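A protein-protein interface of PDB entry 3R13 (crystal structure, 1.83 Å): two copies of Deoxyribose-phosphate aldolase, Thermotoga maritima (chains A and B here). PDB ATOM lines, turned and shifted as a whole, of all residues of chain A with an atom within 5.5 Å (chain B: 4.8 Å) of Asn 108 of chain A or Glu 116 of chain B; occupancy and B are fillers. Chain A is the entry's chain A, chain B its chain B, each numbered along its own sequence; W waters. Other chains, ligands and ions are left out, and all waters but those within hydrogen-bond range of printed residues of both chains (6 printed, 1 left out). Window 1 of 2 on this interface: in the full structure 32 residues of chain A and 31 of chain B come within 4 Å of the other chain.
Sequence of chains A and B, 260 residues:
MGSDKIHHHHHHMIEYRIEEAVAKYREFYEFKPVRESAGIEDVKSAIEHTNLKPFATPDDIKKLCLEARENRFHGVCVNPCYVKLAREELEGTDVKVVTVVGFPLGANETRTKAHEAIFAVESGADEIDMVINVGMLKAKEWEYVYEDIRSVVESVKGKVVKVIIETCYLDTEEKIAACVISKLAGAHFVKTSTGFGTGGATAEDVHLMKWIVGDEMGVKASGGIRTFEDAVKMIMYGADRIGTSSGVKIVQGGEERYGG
The backbone carbonyl oxygen of Ala 107 of chain A sits at hydrogen-bond distance from the backbone NH of Cys 81 of chain B. The side-chain amide nitrogen of Asn 108 of chain A lies within hydrogen-bond range of the side-chain carboxylate of Glu 116 of chain B (2.8 Å). SG of Cys 81 of chain B is in hydrogen-bond range of ND2 of Asn 133 of chain A (3.5 Å).
Leu 105 of chain A touches Phe 103 of chain B (CD1 to CE1, 3.8 Å). Ala 107 of chain A touches Pro 80 of chain B. Cys 81 of chain B touches Asn 108 of chain A. CG of Glu 109 of chain A touches O of Pro 80 of chain B, at 3.8 Å. Phe 119 of chain B touches Glu 109 of chain A (CB to OE1, 3.8 Å). CG2 of Thr 112 of chain A touches OE2 of Glu 116 of chain B, 3.7 Å away. OG1 of Thr 112 of chain A touches CD2 of Phe 119 of chain B (3.4 Å). CB of Cys 81 of chain B touches OH of Tyr 144 of chain A, 3.7 Å away.
Of the 15 printed residues of chain B, 5 touch a printed residue of chain A. Hydrophobic or aromatic side chains of chain B that line the printed part of chain A: Pro 80, Phe 103 and Phe 119. Of the 14 printed residues of chain A, 7 touch a printed residue of chain B. Hydrophobic or aromatic side chains of chain A within 4 Å of the printed part of chain B: Leu 105, Ala 107 and Tyr 144. Among the printed residues, no Asp or Glu carboxylate lies within 4 Å of a Lys or Arg side-chain nitrogen of the other chain.
Positions printed for both chains: 101, 102, 103, 112 and 113.
Water W1 bridges OE2 of Glu 109 of chain A (2.5 Å) and O of Pro 80 of chain B (3.1 Å). Water W6 lies within hydrogen-bond range of the side-chain carboxylate of Glu 116 of chain B (2.6 Å), the side-chain hydroxyl of Thr 112 of chain A (2.8 Å) and the backbone NH of Glu 109 of chain A (2.9 Å). Water W2 lies within hydrogen-bond range of the side-chain carboxylate of Glu 116 of chain B (2.6 Å), the side-chain amide nitrogen of Asn 108 of chain A (3.5 Å) and the backbone NH of Gly 102 of chain B (3.5 Å). Water W3 lies within hydrogen-bond range of O of Phe 103 of chain B (2.7 Å) and ND2 of Asn 108 of chain A (3.1 Å). Water W5 lies within hydrogen-bond range of the backbone carbonyl oxygen (O) of Phe 103 of chain B (2.9 Å), the backbone NH (N) of Leu 105 of chain A (3.0 Å) and the backbone carbonyl oxygen (O) of Phe 103 of chain A (3.2 Å). Water W4 bridges the backbone carbonyl oxygen (O) of Phe 103 of chain A (2.9 Å) and the backbone carbonyl oxygen (O) of Phe 103 of chain B (3.2 Å).
Of the printed residues of chain B, Leu 105 of chain A touches Phe 103. Gly 106 of chain A touches none of the printed residues of chain B. Of chain B, only Cys 81 (3.8 Å) and Glu 116 (2.8 Å) come within 4 Å of Asn 108 of chain A. Of the printed residues of chain B, Asn 133 of chain A touches Cys 81. Val 100 of chain B touches none of the printed residues of chain A. The nearest residue of chain A that does not touch Glu 116 of chain B is Glu 109 of chain A (4.8 Å). The nearest printed residue of chain A that does not touch Pro 80 of chain B is Asn 108 of chain A (4.3 Å).
O of Gly 102 of chain A sits close to OD1 of Asn 108 of chain A (3.5 Å). N of Gly 102 of chain B is in hydrogen-bond range of OE1 of Glu 116 of chain B, at 3.0 Å.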
ATOM      1  N   VAL A 101       4.590  22.863 -21.679  1.00  0.00           N
ATOM      2  CA  VAL A 101       4.250  21.490 -21.329  1.00  0.00           C
ATOM      3  C   VAL A 101       3.349  20.947 -22.401  1.00  0.00           C
ATOM      4  O   VAL A 101       2.373  21.620 -22.814  1.00  0.00           O
ATOM      5  CB  VAL A 101       3.544  21.449 -19.950  1.00  0.00           C
ATOM      6  CG1 VAL A 101       2.757  20.135 -19.731  1.00  0.00           C
ATOM      7  CG2 VAL A 101       4.589  21.677 -18.861  1.00  0.00           C
ATOM      8  N   GLY A 102       3.721  19.773 -22.917  1.00  0.00           N
ATOM      9  CA  GLY A 102       2.949  19.110 -23.966  1.00  0.00           C
ATOM     10  C   GLY A 102       2.990  19.915 -25.234  1.00  0.00           C
ATOM     11  O   GLY A 102       2.010  19.975 -25.985  1.00  0.00           O
ATOM     12  N   PHE A 103       4.136  20.535 -25.479  1.00  0.00           N
ATOM     13  CA  PHE A 103       4.230  21.647 -26.438  1.00  0.00           C
ATOM     14  C   PHE A 103       5.087  21.251 -27.629  1.00  0.00           C
ATOM     15  O   PHE A 103       6.131  20.605 -27.447  1.00  0.00           O
ATOM     16  CB  PHE A 103       4.880  22.810 -25.727  1.00  0.00           C
ATOM     17  CG  PHE A 103       5.092  24.038 -26.575  1.00  0.00           C
ATOM     18  CD1 PHE A 103       6.236  24.160 -27.354  1.00  0.00           C
ATOM     19  CD2 PHE A 103       4.200  25.106 -26.518  1.00  0.00           C
ATOM     20  CE1 PHE A 103       6.449  25.269 -28.133  1.00  0.00           C
ATOM     21  CE2 PHE A 103       4.431  26.231 -27.277  1.00  0.00           C
ATOM     22  CZ  PHE A 103       5.546  26.304 -28.098  1.00  0.00           C
ATOM     23  N   LEU A 105       2.301  20.460 -29.733  1.00  0.00           N
ATOM     24  CA  LEU A 105       1.173  19.748 -30.321  1.00  0.00           C
ATOM     25  C   LEU A 105       0.028  19.397 -29.373  1.00  0.00           C
ATOM     26  O   LEU A 105      -1.074  19.124 -29.846  1.00  0.00           O
ATOM     27  CB  LEU A 105       1.628  18.514 -31.099  1.00  0.00           C
ATOM     28  CG  LEU A 105       2.647  18.760 -32.229  1.00  0.00           C
ATOM     29  CD1 LEU A 105       3.024  17.460 -32.958  1.00  0.00           C
ATOM     30  CD2 LEU A 105       2.201  19.896 -33.192  1.00  0.00           C
ATOM     31  N   GLY A 106       0.286  19.317 -28.066  1.00  0.00           N
ATOM     32  CA  GLY A 106      -0.778  19.074 -27.079  1.00  0.00           C
ATOM     33  C   GLY A 106      -1.355  17.668 -27.111  1.00  0.00           C
ATOM     34  O   GLY A 106      -2.430  17.399 -26.532  1.00  0.00           O
ATOM     35  N   ALA A 107      -0.637  16.754 -27.753  1.00  0.00           N
ATOM     36  CA  ALA A 107      -1.193  15.429 -28.053  1.00  0.00           C
ATOM     37  C   ALA A 107      -0.504  14.308 -27.297  1.00  0.00           C
ATOM     38  O   ALA A 107      -0.644  13.142 -27.688  1.00  0.00           O
ATOM     39  CB  ALA A 107      -1.141  15.170 -29.529  1.00  0.00           C
ATOM     40  N   ASN A 108       0.196  14.672 -26.221  1.00  0.00           N
ATOM     41  CA  ASN A 108       0.744  13.719 -25.254  1.00  0.00           C
ATOM     42  C   ASN A 108      -0.353  13.105 -24.378  1.00  0.00           C
ATOM     43  O   ASN A 108      -1.444  13.671 -24.252  1.00  0.00           O
ATOM     44  CB  ASN A 108       1.758  14.397 -24.339  1.00  0.00           C
ATOM     45  CG  ASN A 108       2.656  15.399 -25.083  1.00  0.00           C
ATOM     46  OD1 ASN A 108       2.248  16.537 -25.390  1.00  0.00           O
ATOM     47  ND2 ASN A 108       3.852  14.976 -25.386  1.00  0.00           N
ATOM     48  N   GLU A 109      -0.045  11.967 -23.749  1.00  0.00           N
ATOM     49  CA  GLU A 109      -0.923  11.387 -22.774  1.00  0.00           C
ATOM     50  C   GLU A 109      -0.989  12.380 -21.639  1.00  0.00           C
ATOM     51  O   GLU A 109       0.002  13.092 -21.330  1.00  0.00           O
ATOM     52  CB  GLU A 109      -0.408  10.035 -22.248  1.00  0.00           C
ATOM     53  CG  GLU A 109      -0.507   8.946 -23.264  1.00  0.00           C
ATOM     54  CD  GLU A 109      -0.397   7.524 -22.674  1.00  0.00           C
ATOM     55  OE1 GLU A 109      -0.202   7.354 -21.449  1.00  0.00           O
ATOM     56  OE2 GLU A 109      -0.516   6.569 -23.462  1.00  0.00           O
ATOM     57  N   THR A 110      -2.151  12.459 -21.039  1.00  0.00           N
ATOM     58  CA  THR A 110      -2.349  13.384 -19.946  1.00  0.00           C
ATOM     59  C   THR A 110      -1.297  13.179 -18.842  1.00  0.00           C
ATOM     60  O   THR A 110      -0.755  14.155 -18.299  1.00  0.00           O
ATOM     61  CB  THR A 110      -3.773  13.221 -19.343  1.00  0.00           C
ATOM     62  OG1 THR A 110      -4.736  13.664 -20.301  1.00  0.00           O
ATOM     63  CG2 THR A 110      -3.894  14.020 -18.068  1.00  0.00           C
ATOM     64  N   THR A 112       1.762  12.192 -19.055  1.00  0.00           N
ATOM     65  CA  THR A 112       3.034  12.773 -19.441  1.00  0.00           C
ATOM     66  C   THR A 112       3.049  14.281 -19.212  1.00  0.00           C
ATOM     67  O   THR A 112       4.056  14.821 -18.742  1.00  0.00           O
ATOM     68  CB  THR A 112       3.333  12.499 -20.907  1.00  0.00           C
ATOM     69  OG1 THR A 112       3.332  11.087 -21.135  1.00  0.00           O
ATOM     70  CG2 THR A 112       4.680  13.154 -21.363  1.00  0.00           C
ATOM     71  N   LYS A 113       1.958  14.962 -19.566  1.00  0.00           N
ATOM     72  CA  LYS A 113       1.838  16.433 -19.329  1.00  0.00           C
ATOM     73  C   LYS A 113       1.985  16.741 -17.835  1.00  0.00           C
ATOM     74  O   LYS A 113       2.716  17.643 -17.428  1.00  0.00           O
ATOM     75  CB  LYS A 113       0.506  17.005 -19.844  1.00  0.00           C
ATOM     76  CG  LYS A 113       0.286  16.891 -21.340  1.00  0.00           C
ATOM     77  CD  LYS A 113      -0.924  17.699 -21.830  1.00  0.00           C
ATOM     78  CE  LYS A 113      -1.250  17.408 -23.303  1.00  0.00           C
ATOM     79  NZ  LYS A 113      -2.401  18.201 -23.811  1.00  0.00           N
ATOM     80  N   ASN A 133      -5.449  19.591 -25.824  1.00  0.00           N
ATOM     81  CA  ASN A 133      -5.583  18.579 -26.854  1.00  0.00           C
ATOM     82  C   ASN A 133      -6.629  19.031 -27.869  1.00  0.00           C
ATOM     83  O   ASN A 133      -7.840  18.858 -27.651  1.00  0.00           O
ATOM     84  CB  ASN A 133      -5.879  17.202 -26.254  1.00  0.00           C
ATOM     85  CG  ASN A 133      -5.710  16.098 -27.257  1.00  0.00           C
ATOM     86  OD1 ASN A 133      -6.186  16.216 -28.386  1.00  0.00           O
ATOM     87  ND2 ASN A 133      -5.006  15.000 -26.859  1.00  0.00           N
ATOM     88  N   TYR A 144     -12.669  14.635 -21.542  1.00  0.00           N
ATOM     89  CA  TYR A 144     -11.231  14.366 -21.774  1.00  0.00           C
ATOM     90  C   TYR A 144     -10.381  15.666 -21.679  1.00  0.00           C
ATOM     91  O   TYR A 144      -9.338  15.702 -21.012  1.00  0.00           O
ATOM     92  CB  TYR A 144     -10.973  13.672 -23.111  1.00  0.00           C
ATOM     93  CG  TYR A 144      -9.500  13.383 -23.334  1.00  0.00           C
ATOM     94  CD1 TYR A 144      -8.651  14.339 -23.859  1.00  0.00           C
ATOM     95  CD2 TYR A 144      -8.954  12.148 -22.980  1.00  0.00           C
ATOM     96  CE1 TYR A 144      -7.278  14.094 -24.038  1.00  0.00           C
ATOM     97  CE2 TYR A 144      -7.597  11.871 -23.168  1.00  0.00           C
ATOM     98  CZ  TYR A 144      -6.764  12.844 -23.707  1.00  0.00           C
ATOM     99  OH  TYR A 144      -5.417  12.571 -23.882  1.00  0.00           O
ATOM    100  N   ASP A 148      -7.559  16.537 -18.867  1.00  0.00           N
ATOM    101  CA  ASP A 148      -6.199  16.756 -19.366  1.00  0.00           C
ATOM    102  C   ASP A 148      -5.622  18.059 -18.755  1.00  0.00           C
ATOM    103  O   ASP A 148      -4.496  18.079 -18.247  1.00  0.00           O
ATOM    104  CB  ASP A 148      -6.265  16.834 -20.881  1.00  0.00           C
ATOM    105  CG  ASP A 148      -4.888  16.855 -21.600  1.00  0.00           C
ATOM    106  OD1 ASP A 148      -4.142  15.835 -21.611  1.00  0.00           O
ATOM    107  OD2 ASP A 148      -4.624  17.875 -22.303  1.00  0.00           O
ATOM    108  N   PRO B  80       1.024  10.308 -28.931  1.00  0.00           N
ATOM    109  CA  PRO B  80       0.894   9.324 -27.868  1.00  0.00           C
ATOM    110  C   PRO B  80      -0.529   9.173 -27.334  1.00  0.00           C
ATOM    111  O   PRO B  80      -0.931   8.067 -26.986  1.00  0.00           O
ATOM    112  CB  PRO B  80       1.854   9.821 -26.792  1.00  0.00           C
ATOM    113  CG  PRO B  80       2.945  10.569 -27.574  1.00  0.00           C
ATOM    114  CD  PRO B  80       2.185  11.206 -28.738  1.00  0.00           C
ATOM    115  N   CYS B  81      -1.305  10.251 -27.277  1.00  0.00           N
ATOM    116  CA  CYS B  81      -2.677  10.173 -26.755  1.00  0.00           C
ATOM    117  C   CYS B  81      -3.556   9.156 -27.495  1.00  0.00           C
ATOM    118  O   CYS B  81      -4.565   8.715 -26.971  1.00  0.00           O
ATOM    119  CB  CYS B  81      -3.361  11.531 -26.780  1.00  0.00           C
ATOM    120  SG  CYS B  81      -3.583  12.239 -28.422  1.00  0.00           S
ATOM    121  N   VAL B 100       5.564   8.963 -31.046  1.00  0.00           N
ATOM    122  CA  VAL B 100       6.655   9.919 -31.050  1.00  0.00           C
ATOM    123  C   VAL B 100       6.884  10.374 -29.637  1.00  0.00           C
ATOM    124  O   VAL B 100       5.943  10.456 -28.843  1.00  0.00           O
ATOM    125  CB  VAL B 100       6.378  11.105 -32.014  1.00  0.00           C
ATOM    126  CG1 VAL B 100       6.409  10.671 -33.503  1.00  0.00           C
ATOM    127  CG2 VAL B 100       4.972  11.855 -31.678  1.00  0.00           C
ATOM    128  N   VAL B 101       8.160  10.646 -29.306  1.00  0.00           N
ATOM    129  CA  VAL B 101       8.582  10.983 -27.968  1.00  0.00           C
ATOM    130  C   VAL B 101       9.438  12.271 -28.013  1.00  0.00           C
ATOM    131  O   VAL B 101      10.322  12.422 -28.875  1.00  0.00           O
ATOM    132  CB  VAL B 101       9.344   9.802 -27.365  1.00  0.00           C
ATOM    133  CG1 VAL B 101      10.096  10.210 -26.124  1.00  0.00           C
ATOM    134  CG2 VAL B 101       8.335   8.674 -27.045  1.00  0.00           C
ATOM    135  N   GLY B 102       9.111  13.214 -27.126  1.00  0.00           N
ATOM    136  CA  GLY B 102       9.792  14.516 -27.076  1.00  0.00           C
ATOM    137  C   GLY B 102       9.658  15.250 -28.387  1.00  0.00           C
ATOM    138  O   GLY B 102      10.606  15.852 -28.873  1.00  0.00           O
ATOM    139  N   PHE B 103       8.472  15.158 -28.985  1.00  0.00           N
ATOM    140  CA  PHE B 103       8.310  15.456 -30.389  1.00  0.00           C
ATOM    141  C   PHE B 103       7.405  16.667 -30.538  1.00  0.00           C
ATOM    142  O   PHE B 103       6.382  16.725 -29.860  1.00  0.00           O
ATOM    143  CB  PHE B 103       7.707  14.230 -31.082  1.00  0.00           C
ATOM    144  CG  PHE B 103       7.387  14.430 -32.533  1.00  0.00           C
ATOM    145  CD1 PHE B 103       6.188  15.031 -32.915  1.00  0.00           C
ATOM    146  CD2 PHE B 103       8.234  13.979 -33.515  1.00  0.00           C
ATOM    147  CE1 PHE B 103       5.881  15.229 -34.251  1.00  0.00           C
ATOM    148  CE2 PHE B 103       7.941  14.165 -34.826  1.00  0.00           C
ATOM    149  CZ  PHE B 103       6.753  14.791 -35.202  1.00  0.00           C
ATOM    150  N   THR B 112      11.578  13.201 -18.823  1.00  0.00           N
ATOM    151  CA  THR B 112      10.263  13.342 -19.411  1.00  0.00           C
ATOM    152  C   THR B 112      10.202  12.468 -20.669  1.00  0.00           C
ATOM    153  O   THR B 112       9.263  11.724 -20.860  1.00  0.00           O
ATOM    154  CB  THR B 112       9.952  14.783 -19.769  1.00  0.00           C
ATOM    155  OG1 THR B 112       9.921  15.571 -18.558  1.00  0.00           O
ATOM    156  CG2 THR B 112       8.608  14.872 -20.543  1.00  0.00           C
ATOM    157  N   LYS B 113      11.226  12.535 -21.511  1.00  0.00           N
ATOM    158  CA  LYS B 113      11.281  11.634 -22.670  1.00  0.00           C
ATOM    159  C   LYS B 113      11.230  10.154 -22.270  1.00  0.00           C
ATOM    160  O   LYS B 113      10.508   9.361 -22.877  1.00  0.00           O
ATOM    161  CB  LYS B 113      12.540  11.882 -23.473  1.00  0.00           C
ATOM    162  CG  LYS B 113      12.606  13.290 -24.070  1.00  0.00           C
ATOM    163  CD  LYS B 113      13.780  13.364 -25.116  1.00  0.00           C
ATOM    164  CE  LYS B 113      14.131  14.783 -25.539  1.00  0.00           C
ATOM    165  NZ  LYS B 113      15.210  14.783 -26.555  1.00  0.00           N
ATOM    166  N   ALA B 114      12.010   9.781 -21.263  1.00  0.00           N
ATOM    167  CA  ALA B 114      12.022   8.380 -20.779  1.00  0.00           C
ATOM    168  C   ALA B 114      10.643   7.958 -20.238  1.00  0.00           C
ATOM    169  O   ALA B 114      10.152   6.866 -20.562  1.00  0.00           O
ATOM    170  CB  ALA B 114      13.129   8.184 -19.714  1.00  0.00           C
ATOM    171  N   HIS B 115       9.990   8.796 -19.435  1.00  0.00           N
ATOM    172  CA  HIS B 115       8.626   8.465 -19.001  1.00  0.00           C
ATOM    173  C   HIS B 115       7.616   8.398 -20.122  1.00  0.00           C
ATOM    174  O   HIS B 115       6.752   7.539 -20.134  1.00  0.00           O
ATOM    175  CB  HIS B 115       8.071   9.434 -17.949  1.00  0.00           C
ATOM    176  CG  HIS B 115       8.700   9.283 -16.598  1.00  0.00           C
ATOM    177  ND1 HIS B 115      10.068   9.258 -16.415  1.00  0.00           N
ATOM    178  CD2 HIS B 115       8.153   9.225 -15.362  1.00  0.00           C
ATOM    179  CE1 HIS B 115      10.330   9.143 -15.124  1.00  0.00           C
ATOM    180  NE2 HIS B 115       9.186   9.113 -14.466  1.00  0.00           N
ATOM    181  N   GLU B 116       7.691   9.328 -21.044  1.00  0.00           N
ATOM    182  CA  GLU B 116       6.767   9.313 -22.149  1.00  0.00           C
ATOM    183  C   GLU B 116       6.909   8.008 -22.929  1.00  0.00           C
ATOM    184  O   GLU B 116       5.890   7.417 -23.368  1.00  0.00           O
ATOM    185  CB  GLU B 116       6.964  10.520 -23.078  1.00  0.00           C
ATOM    186  CG  GLU B 116       6.002  10.506 -24.242  1.00  0.00           C
ATOM    187  CD  GLU B 116       5.795  11.878 -24.917  1.00  0.00           C
ATOM    188  OE1 GLU B 116       6.797  12.457 -25.419  1.00  0.00           O
ATOM    189  OE2 GLU B 116       4.637  12.376 -24.938  1.00  0.00           O
ATOM    190  N   ALA B 117       8.154   7.548 -23.091  1.00  0.00           N
ATOM    191  CA  ALA B 117       8.407   6.291 -23.827  1.00  0.00           C
ATOM    192  C   ALA B 117       7.821   5.076 -23.091  1.00  0.00           C
ATOM    193  O   ALA B 117       7.149   4.240 -23.708  1.00  0.00           O
ATOM    194  CB  ALA B 117       9.929   6.088 -24.097  1.00  0.00           C
ATOM    195  N   ILE B 118       8.065   5.009 -21.784  1.00  0.00           N
ATOM    196  CA  ILE B 118       7.503   3.940 -20.947  1.00  0.00           C
ATOM    197  C   ILE B 118       5.971   3.917 -21.023  1.00  0.00           C
ATOM    198  O   ILE B 118       5.346   2.867 -21.238  1.00  0.00           O
ATOM    199  CB  ILE B 118       7.946   4.085 -19.469  1.00  0.00           C
ATOM    200  CG1 ILE B 118       9.460   3.822 -19.375  1.00  0.00           C
ATOM    201  CG2 ILE B 118       7.152   3.116 -18.568  1.00  0.00           C
ATOM    202  CD1 ILE B 118      10.101   4.282 -18.105  1.00  0.00           C
ATOM    203  N   PHE B 119       5.353   5.078 -20.844  1.00  0.00           N
ATOM    204  CA  PHE B 119       3.904   5.182 -20.930  1.00  0.00           C
ATOM    205  C   PHE B 119       3.373   4.733 -22.305  1.00  0.00           C
ATOM    206  O   PHE B 119       2.381   4.024 -22.376  1.00  0.00           O
ATOM    207  CB  PHE B 119       3.434   6.607 -20.646  1.00  0.00           C
ATOM    208  CG  PHE B 119       3.698   7.107 -19.235  1.00  0.00           C
ATOM    209  CD1 PHE B 119       3.750   6.251 -18.143  1.00  0.00           C
ATOM    210  CD2 PHE B 119       3.782   8.470 -19.003  1.00  0.00           C
ATOM    211  CE1 PHE B 119       3.963   6.741 -16.887  1.00  0.00           C
ATOM    212  CE2 PHE B 119       3.995   8.960 -17.735  1.00  0.00           C
ATOM    213  CZ  PHE B 119       4.078   8.112 -16.684  1.00  0.00           C
ATOM    214  N   ALA B 120       4.036   5.131 -23.376  1.00  0.00           N
ATOM    215  CA  ALA B 120       3.638   4.728 -24.718  1.00  0.00           C
ATOM    216  C   ALA B 120       3.705   3.194 -24.908  1.00  0.00           C
ATOM    217  O   ALA B 120       2.810   2.589 -25.514  1.00  0.00           O
ATOM    218  CB  ALA B 120       4.482   5.419 -25.743  1.00  0.00           C
HETATM  219  O   HOH W   1       1.213   6.661 -25.229  1.00  0.00           O
HETATM  220  O   HOH W   2       7.251  14.944 -24.785  1.00  0.00           O
HETATM  221  O   HOH W   3       6.058  15.986 -27.331  1.00  0.00           O
HETATM  222  O   HOH W   4       8.205  19.071 -28.695  1.00  0.00           O
HETATM  223  O   HOH W   5       4.319  18.443 -28.871  1.00  0.00           O
HETATM  224  O   HOH W   6       2.691  11.028 -23.880  1.00  0.00           O
